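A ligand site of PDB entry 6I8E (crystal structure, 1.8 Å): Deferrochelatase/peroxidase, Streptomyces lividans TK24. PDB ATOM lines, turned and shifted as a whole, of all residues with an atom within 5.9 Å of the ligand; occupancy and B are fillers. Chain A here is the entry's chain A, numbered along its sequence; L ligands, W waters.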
ATOM      1  N   ASN A 179      -8.738  10.560  21.490  1.00  0.00           N
ATOM      2  CA  ASN A 179      -9.742  11.550  21.083  1.00  0.00           C
ATOM      3  C   ASN A 179     -10.806  11.665  22.179  1.00  0.00           C
ATOM      4  O   ASN A 179     -10.719  11.058  23.246  1.00  0.00           O
ATOM      5  CB  ASN A 179     -10.347  11.166  19.723  1.00  0.00           C
ATOM      6  CG  ASN A 179     -10.930   9.768  19.721  1.00  0.00           C
ATOM      7  OD1 ASN A 179     -11.613   9.368  20.684  1.00  0.00           O
ATOM      8  ND2 ASN A 179     -10.702   9.025  18.654  1.00  0.00           N
ATOM      9  N   LEU A 181     -13.804  10.609  22.350  1.00  0.00           N
ATOM     10  CA  LEU A 181     -14.558   9.407  22.649  1.00  0.00           C
ATOM     11  C   LEU A 181     -13.787   8.464  23.566  1.00  0.00           C
ATOM     12  O   LEU A 181     -14.304   7.413  23.953  1.00  0.00           O
ATOM     13  CB  LEU A 181     -14.948   8.675  21.356  1.00  0.00           C
ATOM     14  CG  LEU A 181     -15.703   9.520  20.337  1.00  0.00           C
ATOM     15  CD1 LEU A 181     -16.104   8.679  19.124  1.00  0.00           C
ATOM     16  CD2 LEU A 181     -16.919  10.178  20.962  1.00  0.00           C
ATOM     17  N   PHE A 183     -10.879   6.855  22.911  1.00  0.00           N
ATOM     18  CA  PHE A 183     -10.083   5.826  22.248  1.00  0.00           C
ATOM     19  C   PHE A 183      -8.787   6.411  21.702  1.00  0.00           C
ATOM     20  O   PHE A 183      -8.753   7.550  21.235  1.00  0.00           O
ATOM     21  CB  PHE A 183     -10.853   5.192  21.088  1.00  0.00           C
ATOM     22  CG  PHE A 183     -11.863   4.185  21.525  1.00  0.00           C
ATOM     23  CD1 PHE A 183     -13.075   4.598  22.093  1.00  0.00           C
ATOM     24  CD2 PHE A 183     -11.608   2.826  21.392  1.00  0.00           C
ATOM     25  CE1 PHE A 183     -14.006   3.653  22.515  1.00  0.00           C
ATOM     26  CE2 PHE A 183     -12.554   1.894  21.803  1.00  0.00           C
ATOM     27  CZ  PHE A 183     -13.742   2.314  22.386  1.00  0.00           C
ATOM     28  N   LYS A 184      -7.713   5.607  21.764  1.00  0.00           N
ATOM     29  CA  LYS A 184      -6.483   5.959  21.074  1.00  0.00           C
ATOM     30  C   LYS A 184      -6.763   6.161  19.600  1.00  0.00           C
ATOM     31  O   LYS A 184      -7.529   5.425  18.984  1.00  0.00           O
ATOM     32  CB  LYS A 184      -5.417   4.872  21.238  1.00  0.00           C
ATOM     33  CG  LYS A 184      -4.974   4.644  22.671  1.00  0.00           C
ATOM     34  CD  LYS A 184      -4.016   3.470  22.758  1.00  0.00           C
ATOM     35  CE  LYS A 184      -3.530   3.259  24.183  1.00  0.00           C
ATOM     36  NZ  LYS A 184      -2.530   2.140  24.248  1.00  0.00           N
ATOM     37  N   ASP A 185      -6.097   7.150  19.020  1.00  0.00           N
ATOM     38  CA  ASP A 185      -6.383   7.592  17.663  1.00  0.00           C
ATOM     39  C   ASP A 185      -5.042   7.889  17.028  1.00  0.00           C
ATOM     40  O   ASP A 185      -4.383   8.855  17.408  1.00  0.00           O
ATOM     41  CB  ASP A 185      -7.292   8.827  17.659  1.00  0.00           C
ATOM     42  CG  ASP A 185      -8.098   8.987  16.382  1.00  0.00           C
ATOM     43  OD1 ASP A 185      -7.676   8.480  15.309  1.00  0.00           O
ATOM     44  OD2 ASP A 185      -9.159   9.631  16.456  1.00  0.00           O
ATOM     45  N   GLY A 186      -4.629   7.053  16.066  1.00  0.00           N
ATOM     46  CA  GLY A 186      -3.390   7.303  15.369  1.00  0.00           C
ATOM     47  C   GLY A 186      -2.488   6.073  15.298  1.00  0.00           C
ATOM     48  O   GLY A 186      -1.413   6.135  14.701  1.00  0.00           O
ATOM     49  N   THR A 187      -2.944   4.960  15.875  1.00  0.00           N
ATOM     50  CA  THR A 187      -2.125   3.751  15.953  1.00  0.00           C
ATOM     51  C   THR A 187      -1.589   3.327  14.580  1.00  0.00           C
ATOM     52  O   THR A 187      -0.375   3.232  14.367  1.00  0.00           O
ATOM     53  CB  THR A 187      -2.933   2.629  16.602  1.00  0.00           C
ATOM     54  OG1 THR A 187      -3.316   3.045  17.915  1.00  0.00           O
ATOM     55  CG2 THR A 187      -2.131   1.342  16.688  1.00  0.00           C
ATOM     56  N   ARG A 188      -2.482   3.049  13.628  1.00  0.00           N
ATOM     57  CA  ARG A 188      -2.070   2.615  12.292  1.00  0.00           C
ATOM     58  C   ARG A 188      -2.215   3.791  11.326  1.00  0.00           C
ATOM     59  O   ARG A 188      -3.177   3.929  10.579  1.00  0.00           O
ATOM     60  CB  ARG A 188      -2.872   1.394  11.832  1.00  0.00           C
ATOM     61  CG  ARG A 188      -2.384   0.078  12.496  1.00  0.00           C
ATOM     62  CD  ARG A 188      -3.151  -1.140  11.966  1.00  0.00           C
ATOM     63  NE  ARG A 188      -3.553  -0.898  10.598  1.00  0.00           N
ATOM     64  CZ  ARG A 188      -2.757  -1.085   9.549  1.00  0.00           C
ATOM     65  NH1 ARG A 188      -3.194  -0.791   8.334  1.00  0.00           N
ATOM     66  NH2 ARG A 188      -1.531  -1.577   9.730  1.00  0.00           N
ATOM     67  N   ASN A 189      -1.222   4.660  11.388  1.00  0.00           N
ATOM     68  CA  ASN A 189      -1.093   5.810  10.520  1.00  0.00           C
ATOM     69  C   ASN A 189       0.209   5.606   9.755  1.00  0.00           C
ATOM     70  O   ASN A 189       0.819   4.543   9.824  1.00  0.00           O
ATOM     71  CB  ASN A 189      -1.149   7.085  11.357  1.00  0.00           C
ATOM     72  CG  ASN A 189      -1.485   8.314  10.548  1.00  0.00           C
ATOM     73  OD1 ASN A 189      -2.321   8.264   9.646  1.00  0.00           O
ATOM     74  ND2 ASN A 189      -0.842   9.416  10.877  1.00  0.00           N
ATOM     75  N   ILE A 224     -15.899  17.654  12.339  1.00  0.00           N
ATOM     76  CA  ILE A 224     -16.806  16.572  12.690  1.00  0.00           C
ATOM     77  C   ILE A 224     -17.312  16.794  14.107  1.00  0.00           C
ATOM     78  O   ILE A 224     -16.523  16.766  15.066  1.00  0.00           O
ATOM     79  CB  ILE A 224     -16.158  15.186  12.547  1.00  0.00           C
ATOM     80  CG1 ILE A 224     -15.569  15.028  11.144  1.00  0.00           C
ATOM     81  CG2 ILE A 224     -17.193  14.091  12.819  1.00  0.00           C
ATOM     82  CD1 ILE A 224     -14.733  13.745  10.986  1.00  0.00           C
ATOM     83  N   ARG A 225     -18.616  16.979  14.245  1.00  0.00           N
ATOM     84  CA  ARG A 225     -19.226  17.046  15.572  1.00  0.00           C
ATOM     85  C   ARG A 225     -19.423  15.643  16.119  1.00  0.00           C
ATOM     86  O   ARG A 225     -19.756  14.714  15.385  1.00  0.00           O
ATOM     87  CB  ARG A 225     -20.575  17.766  15.508  1.00  0.00           C
ATOM     88  CG  ARG A 225     -21.292  17.852  16.859  1.00  0.00           C
ATOM     89  CD  ARG A 225     -22.623  18.579  16.708  1.00  0.00           C
ATOM     90  NE  ARG A 225     -22.478  19.737  15.839  1.00  0.00           N
ATOM     91  CZ  ARG A 225     -22.019  20.921  16.232  1.00  0.00           C
ATOM     92  NH1 ARG A 225     -21.655  21.098  17.495  1.00  0.00           N
ATOM     93  NH2 ARG A 225     -21.916  21.923  15.364  1.00  0.00           N
ATOM     94  N   MET A 226     -19.229  15.505  17.428  1.00  0.00           N
ATOM     95  CA  MET A 226     -19.447  14.266  18.165  1.00  0.00           C
ATOM     96  C   MET A 226     -20.683  14.392  19.051  1.00  0.00           C
ATOM     97  O   MET A 226     -20.809  15.373  19.793  1.00  0.00           O
ATOM     98  CB  MET A 226     -18.223  13.940  19.020  1.00  0.00           C
ATOM     99  CG  MET A 226     -16.985  13.631  18.201  1.00  0.00           C
ATOM    100  SD  MET A 226     -15.585  13.489  19.335  1.00  0.00           S
ATOM    101  CE  MET A 226     -14.397  12.725  18.246  1.00  0.00           C
ATOM    102  N   PHE A 243     -15.716   0.367  17.195  1.00  0.00           N
ATOM    103  CA  PHE A 243     -14.397   0.551  16.633  1.00  0.00           C
ATOM    104  C   PHE A 243     -13.715  -0.748  16.206  1.00  0.00           C
ATOM    105  O   PHE A 243     -13.002  -0.763  15.210  1.00  0.00           O
ATOM    106  CB  PHE A 243     -13.503   1.308  17.609  1.00  0.00           C
ATOM    107  CG  PHE A 243     -13.774   2.772  17.610  1.00  0.00           C
ATOM    108  CD1 PHE A 243     -13.464   3.526  16.475  1.00  0.00           C
ATOM    109  CD2 PHE A 243     -14.391   3.387  18.684  1.00  0.00           C
ATOM    110  CE1 PHE A 243     -13.734   4.888  16.440  1.00  0.00           C
ATOM    111  CE2 PHE A 243     -14.670   4.753  18.647  1.00  0.00           C
ATOM    112  CZ  PHE A 243     -14.337   5.489  17.525  1.00  0.00           C
ATOM    113  N   ARG A 245     -11.627  -2.203  18.423  1.00  0.00           N
ATOM    114  CA  ARG A 245     -10.483  -2.265  19.312  1.00  0.00           C
ATOM    115  C   ARG A 245     -11.018  -2.061  20.717  1.00  0.00           C
ATOM    116  O   ARG A 245     -12.073  -1.456  20.908  1.00  0.00           O
ATOM    117  CB  ARG A 245      -9.431  -1.195  18.996  1.00  0.00           C
ATOM    118  CG  ARG A 245      -8.665  -1.382  17.669  1.00  0.00           C
ATOM    119  CD  ARG A 245      -7.735  -0.187  17.434  1.00  0.00           C
ATOM    120  NE  ARG A 245      -6.914  -0.311  16.221  1.00  0.00           N
ATOM    121  CZ  ARG A 245      -5.696  -0.852  16.180  1.00  0.00           C
ATOM    122  NH1 ARG A 245      -5.154  -1.342  17.276  1.00  0.00           N
ATOM    123  NH2 ARG A 245      -5.027  -0.895  15.034  1.00  0.00           N
ATOM    124  N   PRO A 262      -4.508  -5.889  13.348  1.00  0.00           N
ATOM    125  CA  PRO A 262      -5.917  -6.274  13.410  1.00  0.00           C
ATOM    126  C   PRO A 262      -6.172  -7.518  12.573  1.00  0.00           C
ATOM    127  O   PRO A 262      -5.585  -7.706  11.502  1.00  0.00           O
ATOM    128  CB  PRO A 262      -6.647  -5.048  12.856  1.00  0.00           C
ATOM    129  CG  PRO A 262      -5.644  -4.271  12.141  1.00  0.00           C
ATOM    130  CD  PRO A 262      -4.313  -4.542  12.790  1.00  0.00           C
ATOM    131  N   HIS A 272     -15.596   0.468  12.563  1.00  0.00           N
ATOM    132  CA  HIS A 272     -14.905   1.550  11.900  1.00  0.00           C
ATOM    133  C   HIS A 272     -13.538   1.118  11.354  1.00  0.00           C
ATOM    134  O   HIS A 272     -13.182   1.430  10.214  1.00  0.00           O
ATOM    135  CB  HIS A 272     -14.758   2.713  12.876  1.00  0.00           C
ATOM    136  CG  HIS A 272     -14.019   3.885  12.314  1.00  0.00           C
ATOM    137  ND1 HIS A 272     -14.599   4.770  11.437  1.00  0.00           N
ATOM    138  CD2 HIS A 272     -12.764   4.325  12.527  1.00  0.00           C
ATOM    139  CE1 HIS A 272     -13.723   5.703  11.107  1.00  0.00           C
ATOM    140  NE2 HIS A 272     -12.595   5.457  11.766  1.00  0.00           N
ATOM    141  N   VAL A 273     -12.762   0.403  12.159  1.00  0.00           N
ATOM    142  CA  VAL A 273     -11.435  -0.009  11.708  1.00  0.00           C
ATOM    143  C   VAL A 273     -11.556  -0.976  10.547  1.00  0.00           C
ATOM    144  O   VAL A 273     -10.793  -0.899   9.578  1.00  0.00           O
ATOM    145  CB  VAL A 273     -10.644  -0.638  12.872  1.00  0.00           C
ATOM    146  CG1 VAL A 273      -9.386  -1.319  12.327  1.00  0.00           C
ATOM    147  CG2 VAL A 273     -10.284   0.433  13.853  1.00  0.00           C
ATOM    148  N   ALA A 276     -12.332   1.143   7.451  1.00  0.00           N
ATOM    149  CA  ALA A 276     -11.329   2.130   7.061  1.00  0.00           C
ATOM    150  C   ALA A 276      -9.999   1.509   6.661  1.00  0.00           C
ATOM    151  O   ALA A 276      -9.189   2.198   6.031  1.00  0.00           O
ATOM    152  CB  ALA A 276     -11.117   3.135   8.199  1.00  0.00           C
ATOM    153  N   HIS A 277      -9.777   0.248   6.998  1.00  0.00           N
ATOM    154  CA  HIS A 277      -8.489  -0.390   6.794  1.00  0.00           C
ATOM    155  C   HIS A 277      -8.124  -0.392   5.307  1.00  0.00           C
ATOM    156  O   HIS A 277      -8.995  -0.569   4.451  1.00  0.00           O
ATOM    157  CB  HIS A 277      -8.545  -1.824   7.351  1.00  0.00           C
ATOM    158  CG  HIS A 277      -7.200  -2.481   7.488  1.00  0.00           C
ATOM    159  ND1 HIS A 277      -6.501  -2.990   6.427  1.00  0.00           N
ATOM    160  CD2 HIS A 277      -6.436  -2.722   8.584  1.00  0.00           C
ATOM    161  CE1 HIS A 277      -5.355  -3.497   6.837  1.00  0.00           C
ATOM    162  NE2 HIS A 277      -5.295  -3.347   8.157  1.00  0.00           N
ATOM    163  N   PRO A 278      -6.842  -0.183   4.969  1.00  0.00           N
ATOM    164  CA  PRO A 278      -6.453  -0.249   3.555  1.00  0.00           C
ATOM    165  C   PRO A 278      -6.888  -1.537   2.860  1.00  0.00           C
ATOM    166  O   PRO A 278      -7.329  -1.489   1.696  1.00  0.00           O
ATOM    167  CB  PRO A 278      -4.914  -0.133   3.617  1.00  0.00           C
ATOM    168  CG  PRO A 278      -4.652   0.661   4.852  1.00  0.00           C
ATOM    169  CD  PRO A 278      -5.744   0.282   5.839  1.00  0.00           C
ATOM    170  N   LEU A 286      -4.025   6.660   4.171  1.00  0.00           N
ATOM    171  CA  LEU A 286      -4.081   8.079   4.493  1.00  0.00           C
ATOM    172  C   LEU A 286      -3.066   8.420   5.564  1.00  0.00           C
ATOM    173  O   LEU A 286      -2.701   7.579   6.381  1.00  0.00           O
ATOM    174  CB  LEU A 286      -5.460   8.483   5.029  1.00  0.00           C
ATOM    175  CG  LEU A 286      -6.621   8.195   4.110  1.00  0.00           C
ATOM    176  CD1 LEU A 286      -7.927   8.454   4.855  1.00  0.00           C
ATOM    177  CD2 LEU A 286      -6.478   9.057   2.876  1.00  0.00           C
ATOM    178  N   ARG A 288      -3.318  10.650   8.600  1.00  0.00           N
ATOM    179  CA  ARG A 288      -4.224  11.418   9.433  1.00  0.00           C
ATOM    180  C   ARG A 288      -3.450  12.313  10.386  1.00  0.00           C
ATOM    181  O   ARG A 288      -2.460  11.879  10.995  1.00  0.00           O
ATOM    182  CB  ARG A 288      -5.154  10.487  10.214  1.00  0.00           C
ATOM    183  CG  ARG A 288      -6.164   9.784   9.342  1.00  0.00           C
ATOM    184  CD  ARG A 288      -6.905   8.704  10.109  1.00  0.00           C
ATOM    185  NE  ARG A 288      -6.042   7.564  10.386  1.00  0.00           N
ATOM    186  CZ  ARG A 288      -5.928   6.962  11.570  1.00  0.00           C
ATOM    187  NH1 ARG A 288      -6.639   7.371  12.615  1.00  0.00           N
ATOM    188  NH2 ARG A 288      -5.090   5.932  11.714  1.00  0.00           N
ATOM    189  N   LEU A 307     -14.080  16.650  16.419  1.00  0.00           N
ATOM    190  CA  LEU A 307     -12.765  16.306  15.903  1.00  0.00           C
ATOM    191  C   LEU A 307     -12.585  17.056  14.593  1.00  0.00           C
ATOM    192  O   LEU A 307     -13.437  16.976  13.703  1.00  0.00           O
ATOM    193  CB  LEU A 307     -12.613  14.803  15.699  1.00  0.00           C
ATOM    194  CG  LEU A 307     -11.207  14.304  15.395  1.00  0.00           C
ATOM    195  CD1 LEU A 307     -11.025  12.874  15.887  1.00  0.00           C
ATOM    196  CD2 LEU A 307     -10.915  14.401  13.896  1.00  0.00           C
ATOM    197  N   PHE A 309     -10.802  16.783  11.603  1.00  0.00           N
ATOM    198  CA  PHE A 309     -10.106  15.718  10.897  1.00  0.00           C
ATOM    199  C   PHE A 309      -9.283  16.294   9.740  1.00  0.00           C
ATOM    200  O   PHE A 309      -9.791  17.073   8.934  1.00  0.00           O
ATOM    201  CB  PHE A 309     -11.146  14.708  10.391  1.00  0.00           C
ATOM    202  CG  PHE A 309     -10.558  13.523   9.651  1.00  0.00           C
ATOM    203  CD1 PHE A 309     -10.205  12.375  10.328  1.00  0.00           C
ATOM    204  CD2 PHE A 309     -10.415  13.566   8.276  1.00  0.00           C
ATOM    205  CE1 PHE A 309      -9.670  11.281   9.631  1.00  0.00           C
ATOM    206  CE2 PHE A 309      -9.891  12.493   7.574  1.00  0.00           C
ATOM    207  CZ  PHE A 309      -9.527  11.348   8.259  1.00  0.00           C
ATOM    208  N   PHE A 320      -8.885   9.877   0.407  1.00  0.00           N
ATOM    209  CA  PHE A 320     -10.024  10.128   1.275  1.00  0.00           C
ATOM    210  C   PHE A 320     -11.333   9.660   0.644  1.00  0.00           C
ATOM    211  O   PHE A 320     -12.185   9.089   1.326  1.00  0.00           O
ATOM    212  CB  PHE A 320     -10.081  11.623   1.617  1.00  0.00           C
ATOM    213  CG  PHE A 320     -11.297  12.036   2.409  1.00  0.00           C
ATOM    214  CD1 PHE A 320     -11.283  11.972   3.792  1.00  0.00           C
ATOM    215  CD2 PHE A 320     -12.435  12.499   1.762  1.00  0.00           C
ATOM    216  CE1 PHE A 320     -12.405  12.352   4.532  1.00  0.00           C
ATOM    217  CE2 PHE A 320     -13.563  12.888   2.492  1.00  0.00           C
ATOM    218  CZ  PHE A 320     -13.554  12.808   3.864  1.00  0.00           C
ATOM    219  N   VAL A 323     -12.119   5.806   0.945  1.00  0.00           N
ATOM    220  CA  VAL A 323     -12.265   5.417   2.349  1.00  0.00           C
ATOM    221  C   VAL A 323     -13.563   5.978   2.915  1.00  0.00           C
ATOM    222  O   VAL A 323     -14.364   5.257   3.531  1.00  0.00           O
ATOM    223  CB  VAL A 323     -11.045   5.847   3.191  1.00  0.00           C
ATOM    224  CG1 VAL A 323     -11.214   5.383   4.652  1.00  0.00           C
ATOM    225  CG2 VAL A 323      -9.741   5.298   2.622  1.00  0.00           C
ATOM    226  N   GLN A 324     -13.824   7.273   2.706  1.00  0.00           N
ATOM    227  CA  GLN A 324     -15.049   7.856   3.244  1.00  0.00           C
ATOM    228  C   GLN A 324     -16.277   7.222   2.589  1.00  0.00           C
ATOM    229  O   GLN A 324     -17.298   7.015   3.249  1.00  0.00           O
ATOM    230  CB  GLN A 324     -15.053   9.372   3.072  1.00  0.00           C
ATOM    231  CG  GLN A 324     -16.347  10.073   3.487  1.00  0.00           C
ATOM    232  CD  GLN A 324     -16.608  10.065   4.991  1.00  0.00           C
ATOM    233  OE1 GLN A 324     -15.690  10.017   5.797  1.00  0.00           O
ATOM    234  NE2 GLN A 324     -17.874  10.135   5.366  1.00  0.00           N
ATOM    235  N   LEU A 327     -17.161   4.249   4.437  1.00  0.00           N
ATOM    236  CA  LEU A 327     -17.699   4.466   5.773  1.00  0.00           C
ATOM    237  C   LEU A 327     -19.198   4.759   5.774  1.00  0.00           C
ATOM    238  O   LEU A 327     -19.743   5.138   6.815  1.00  0.00           O
ATOM    239  CB  LEU A 327     -16.937   5.596   6.474  1.00  0.00           C
ATOM    240  CG  LEU A 327     -15.424   5.420   6.587  1.00  0.00           C
ATOM    241  CD1 LEU A 327     -14.822   6.576   7.380  1.00  0.00           C
ATOM    242  CD2 LEU A 327     -15.055   4.079   7.219  1.00  0.00           C
ATOM    243  N   LEU A 332     -19.832   4.060  13.507  1.00  0.00           N
ATOM    244  CA  LEU A 332     -19.529   5.334  14.146  1.00  0.00           C
ATOM    245  C   LEU A 332     -20.476   6.446  13.688  1.00  0.00           C
ATOM    246  O   LEU A 332     -20.620   7.446  14.396  1.00  0.00           O
ATOM    247  CB  LEU A 332     -18.080   5.726  13.868  1.00  0.00           C
ATOM    248  CG  LEU A 332     -17.519   7.035  14.409  1.00  0.00           C
ATOM    249  CD1 LEU A 332     -17.490   7.003  15.931  1.00  0.00           C
ATOM    250  CD2 LEU A 332     -16.124   7.239  13.855  1.00  0.00           C
ATOM    251  N   ILE A 336     -21.539  10.758  15.117  1.00  0.00           N
ATOM    252  CA  ILE A 336     -20.775  11.874  14.582  1.00  0.00           C
ATOM    253  C   ILE A 336     -21.587  12.522  13.470  1.00  0.00           C
ATOM    254  O   ILE A 336     -22.533  11.935  12.947  1.00  0.00           O
ATOM    255  CB  ILE A 336     -19.397  11.420  14.042  1.00  0.00           C
ATOM    256  CG1 ILE A 336     -19.550  10.381  12.923  1.00  0.00           C
ATOM    257  CG2 ILE A 336     -18.552  10.872  15.178  1.00  0.00           C
ATOM    258  CD1 ILE A 336     -18.338  10.282  11.993  1.00  0.00           C
ATOM    259  N   HIS A 338     -20.563  15.248  10.098  1.00  0.00           N
ATOM    260  CA  HIS A 338     -19.636  16.131   9.399  1.00  0.00           C
ATOM    261  C   HIS A 338     -20.351  17.452   9.160  1.00  0.00           C
ATOM    262  O   HIS A 338     -21.429  17.475   8.565  1.00  0.00           O
ATOM    263  CB  HIS A 338     -19.191  15.512   8.068  1.00  0.00           C
ATOM    264  CG  HIS A 338     -18.349  14.277   8.203  1.00  0.00           C
ATOM    265  ND1 HIS A 338     -17.102  14.164   7.619  1.00  0.00           N
ATOM    266  CD2 HIS A 338     -18.596  13.094   8.810  1.00  0.00           C
ATOM    267  CE1 HIS A 338     -16.605  12.961   7.891  1.00  0.00           C
ATOM    268  NE2 HIS A 338     -17.494  12.301   8.604  1.00  0.00           N
HETATM  269  C1  LIG L   1      -8.575   4.343  12.707  1.00  0.00           C
HETATM  270  C2  LIG L   1     -11.439   7.146  15.426  1.00  0.00           C
HETATM  271  C3  LIG L   1     -12.939   9.540  11.497  1.00  0.00           C
HETATM  272  C4  LIG L   1     -10.011   6.801   8.784  1.00  0.00           C
HETATM  273  C5  LIG L   1      -9.236   4.867  13.782  1.00  0.00           C
HETATM  274  C6  LIG L   1      -9.126   4.413  15.152  1.00  0.00           C
HETATM  275  C7  LIG L   1      -9.935   5.165  15.894  1.00  0.00           C
HETATM  276  C8  LIG L   1     -10.559   6.155  15.036  1.00  0.00           C
HETATM  277  C9  LIG L   1     -10.150   5.048  17.417  1.00  0.00           C
HETATM  278  C10 LIG L   1      -8.252   3.213  15.587  1.00  0.00           C
HETATM  279  C11 LIG L   1      -6.819   3.622  15.913  1.00  0.00           C
HETATM  280  C12 LIG L   1      -6.002   4.085  14.736  1.00  0.00           C
HETATM  281  O1  LIG L   1      -5.422   3.203  14.049  1.00  0.00           O
HETATM  282  O2  LIG L   1      -5.884   5.318  14.502  1.00  0.00           O
HETATM  283  C13 LIG L   1     -12.080   8.039  14.601  1.00  0.00           C
HETATM  284  C14 LIG L   1     -13.012   9.056  15.032  1.00  0.00           C
HETATM  285  C15 LIG L   1     -13.462   9.717  13.943  1.00  0.00           C
HETATM  286  C16 LIG L   1     -12.794   9.137  12.801  1.00  0.00           C
HETATM  287  C17 LIG L   1     -13.415   9.277  16.508  1.00  0.00           C
HETATM  288  C18 LIG L   1     -14.447  10.907  13.865  1.00  0.00           C
HETATM  289  C19 LIG L   1     -14.772  11.635  14.928  1.00  0.00           C
HETATM  290  C20 LIG L   1     -12.276   8.999  10.426  1.00  0.00           C
HETATM  291  C21 LIG L   1     -12.467   9.372   9.045  1.00  0.00           C
HETATM  292  C22 LIG L   1     -11.657   8.618   8.289  1.00  0.00           C
HETATM  293  C23 LIG L   1     -10.944   7.732   9.176  1.00  0.00           C
HETATM  294  C24 LIG L   1     -13.450  10.494   8.627  1.00  0.00           C
HETATM  295  C25 LIG L   1     -11.497   8.617   6.759  1.00  0.00           C
HETATM  296  C26 LIG L   1     -12.404   9.212   5.984  1.00  0.00           C
HETATM  297  C27 LIG L   1      -9.345   5.937   9.612  1.00  0.00           C
HETATM  298  C28 LIG L   1      -8.272   5.060   9.204  1.00  0.00           C
HETATM  299  C29 LIG L   1      -7.879   4.371  10.288  1.00  0.00           C
HETATM  300  C30 LIG L   1      -8.671   4.802  11.410  1.00  0.00           C
HETATM  301  C31 LIG L   1      -7.739   4.954   7.758  1.00  0.00           C
HETATM  302  C32 LIG L   1      -6.767   3.300  10.358  1.00  0.00           C
HETATM  303  C33 LIG L   1      -7.383   1.949  10.018  1.00  0.00           C
HETATM  304  C34 LIG L   1      -6.289   0.933   9.887  1.00  0.00           C
HETATM  305  O3  LIG L   1      -5.561   0.986   8.862  1.00  0.00           O
HETATM  306  O4  LIG L   1      -6.144   0.096  10.817  1.00  0.00           O
HETATM  307  N1  LIG L   1     -10.118   5.941  13.757  1.00  0.00           N
HETATM  308  N2  LIG L   1     -11.956   8.118  13.239  1.00  0.00           N
HETATM  309  N3  LIG L   1     -11.346   7.985  10.471  1.00  0.00           N
HETATM  310  N4  LIG L   1      -9.558   5.765  10.965  1.00  0.00           N
HETATM  311 FE1  LIG L   1     -10.885   6.880  12.088  1.00  0.00          FE
HETATM  312  O   HOH W   1      -7.103   3.707   4.848  1.00  0.00           O
HETATM  313  O   HOH W   2      -4.936   4.648   6.193  1.00  0.00           O
HETATM  314  O   HOH W   3      -6.632   0.600  13.589  1.00  0.00           O
HETATM  315  O   HOH W   4      -3.898   2.879   7.953  1.00  0.00           O
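Water W4 bridges O3 of the ligand and O of Arg 188. Water W3 bridges NH2 of Arg 245 (2.6 Å) and O4 of the ligand (2.9 Å).
NE2 of His 272 binds FE1 of the ligand (2.2 Å). N of Gly 186 is in hydrogen-bond range of O2 of the ligand (2.7 Å). An oxygen (O1) of the ligand lies within hydrogen-bond range of the backbone NH (N) of Arg 188 (3.0 Å). The guanidinium group (NE) of Arg 188 is in salt-bridge range of an oxygen (O4) of the ligand (2.8 Å). The guanidinium group of Arg 288 is in salt-bridge range of an oxygen (O2) of the ligand. The backbone NH of Thr 187 is in hydrogen-bond range of an oxygen (O2) of the ligand (3.3 Å).
O of Arg 188 is in hydrogen-bond range of NH2 of Arg 288. The guanidinium group (NH1) of Arg 188 sits at hydrogen-bond distance from a ring nitrogen (NE2) of His 277, 3.3 Å away. The guanidinium group of Arg 288 is in salt-bridge range of the side-chain carboxylate of Asp 185. O of Phe 243 sits close to N of Val 273, 3.3 Å away. The side-chain carboxylate (OD2) of Asp 185 lies within hydrogen-bond range of the side-chain amide nitrogen (ND2) of Asn 179, 2.8 Å away. The backbone carbonyl oxygen of Phe 183 sits close to the side-chain amide oxygen of Asn 179. OD1 of Asn 179 is in hydrogen-bond range of N of Leu 181 (3.0 Å). N of Leu 307 is in hydrogen-bond range of O of Ile 224, 2.8 Å away.
Residues that only touch the ligand: Lys 184, Pro 278, Phe 243, Gln 324, Phe 309, Phe 320, Asn 179, Met 226, Asp 185, Ala 276, His 277, Leu 332, Phe 183, Leu 181, Arg 245, Leu 327, Val 273, Ile 336, Val 323 and Leu 307. 25 residues have an atom within 4 Å of the ligand: Asn 179, Leu 181, Phe 183, Lys 184, Asp 185, Gly 186, Thr 187, Arg 188, Met 226, Phe 243, Arg 245, His 272, Val 273, Ala 276, His 277, Pro 278, Arg 288, Leu 307, Phe 309, Phe 320, Val 323, Gln 324, Leu 327, Leu 332 and Ile 336. The nearest printed residue that does not touch the ligand is Ile 224 (4.04 Å).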
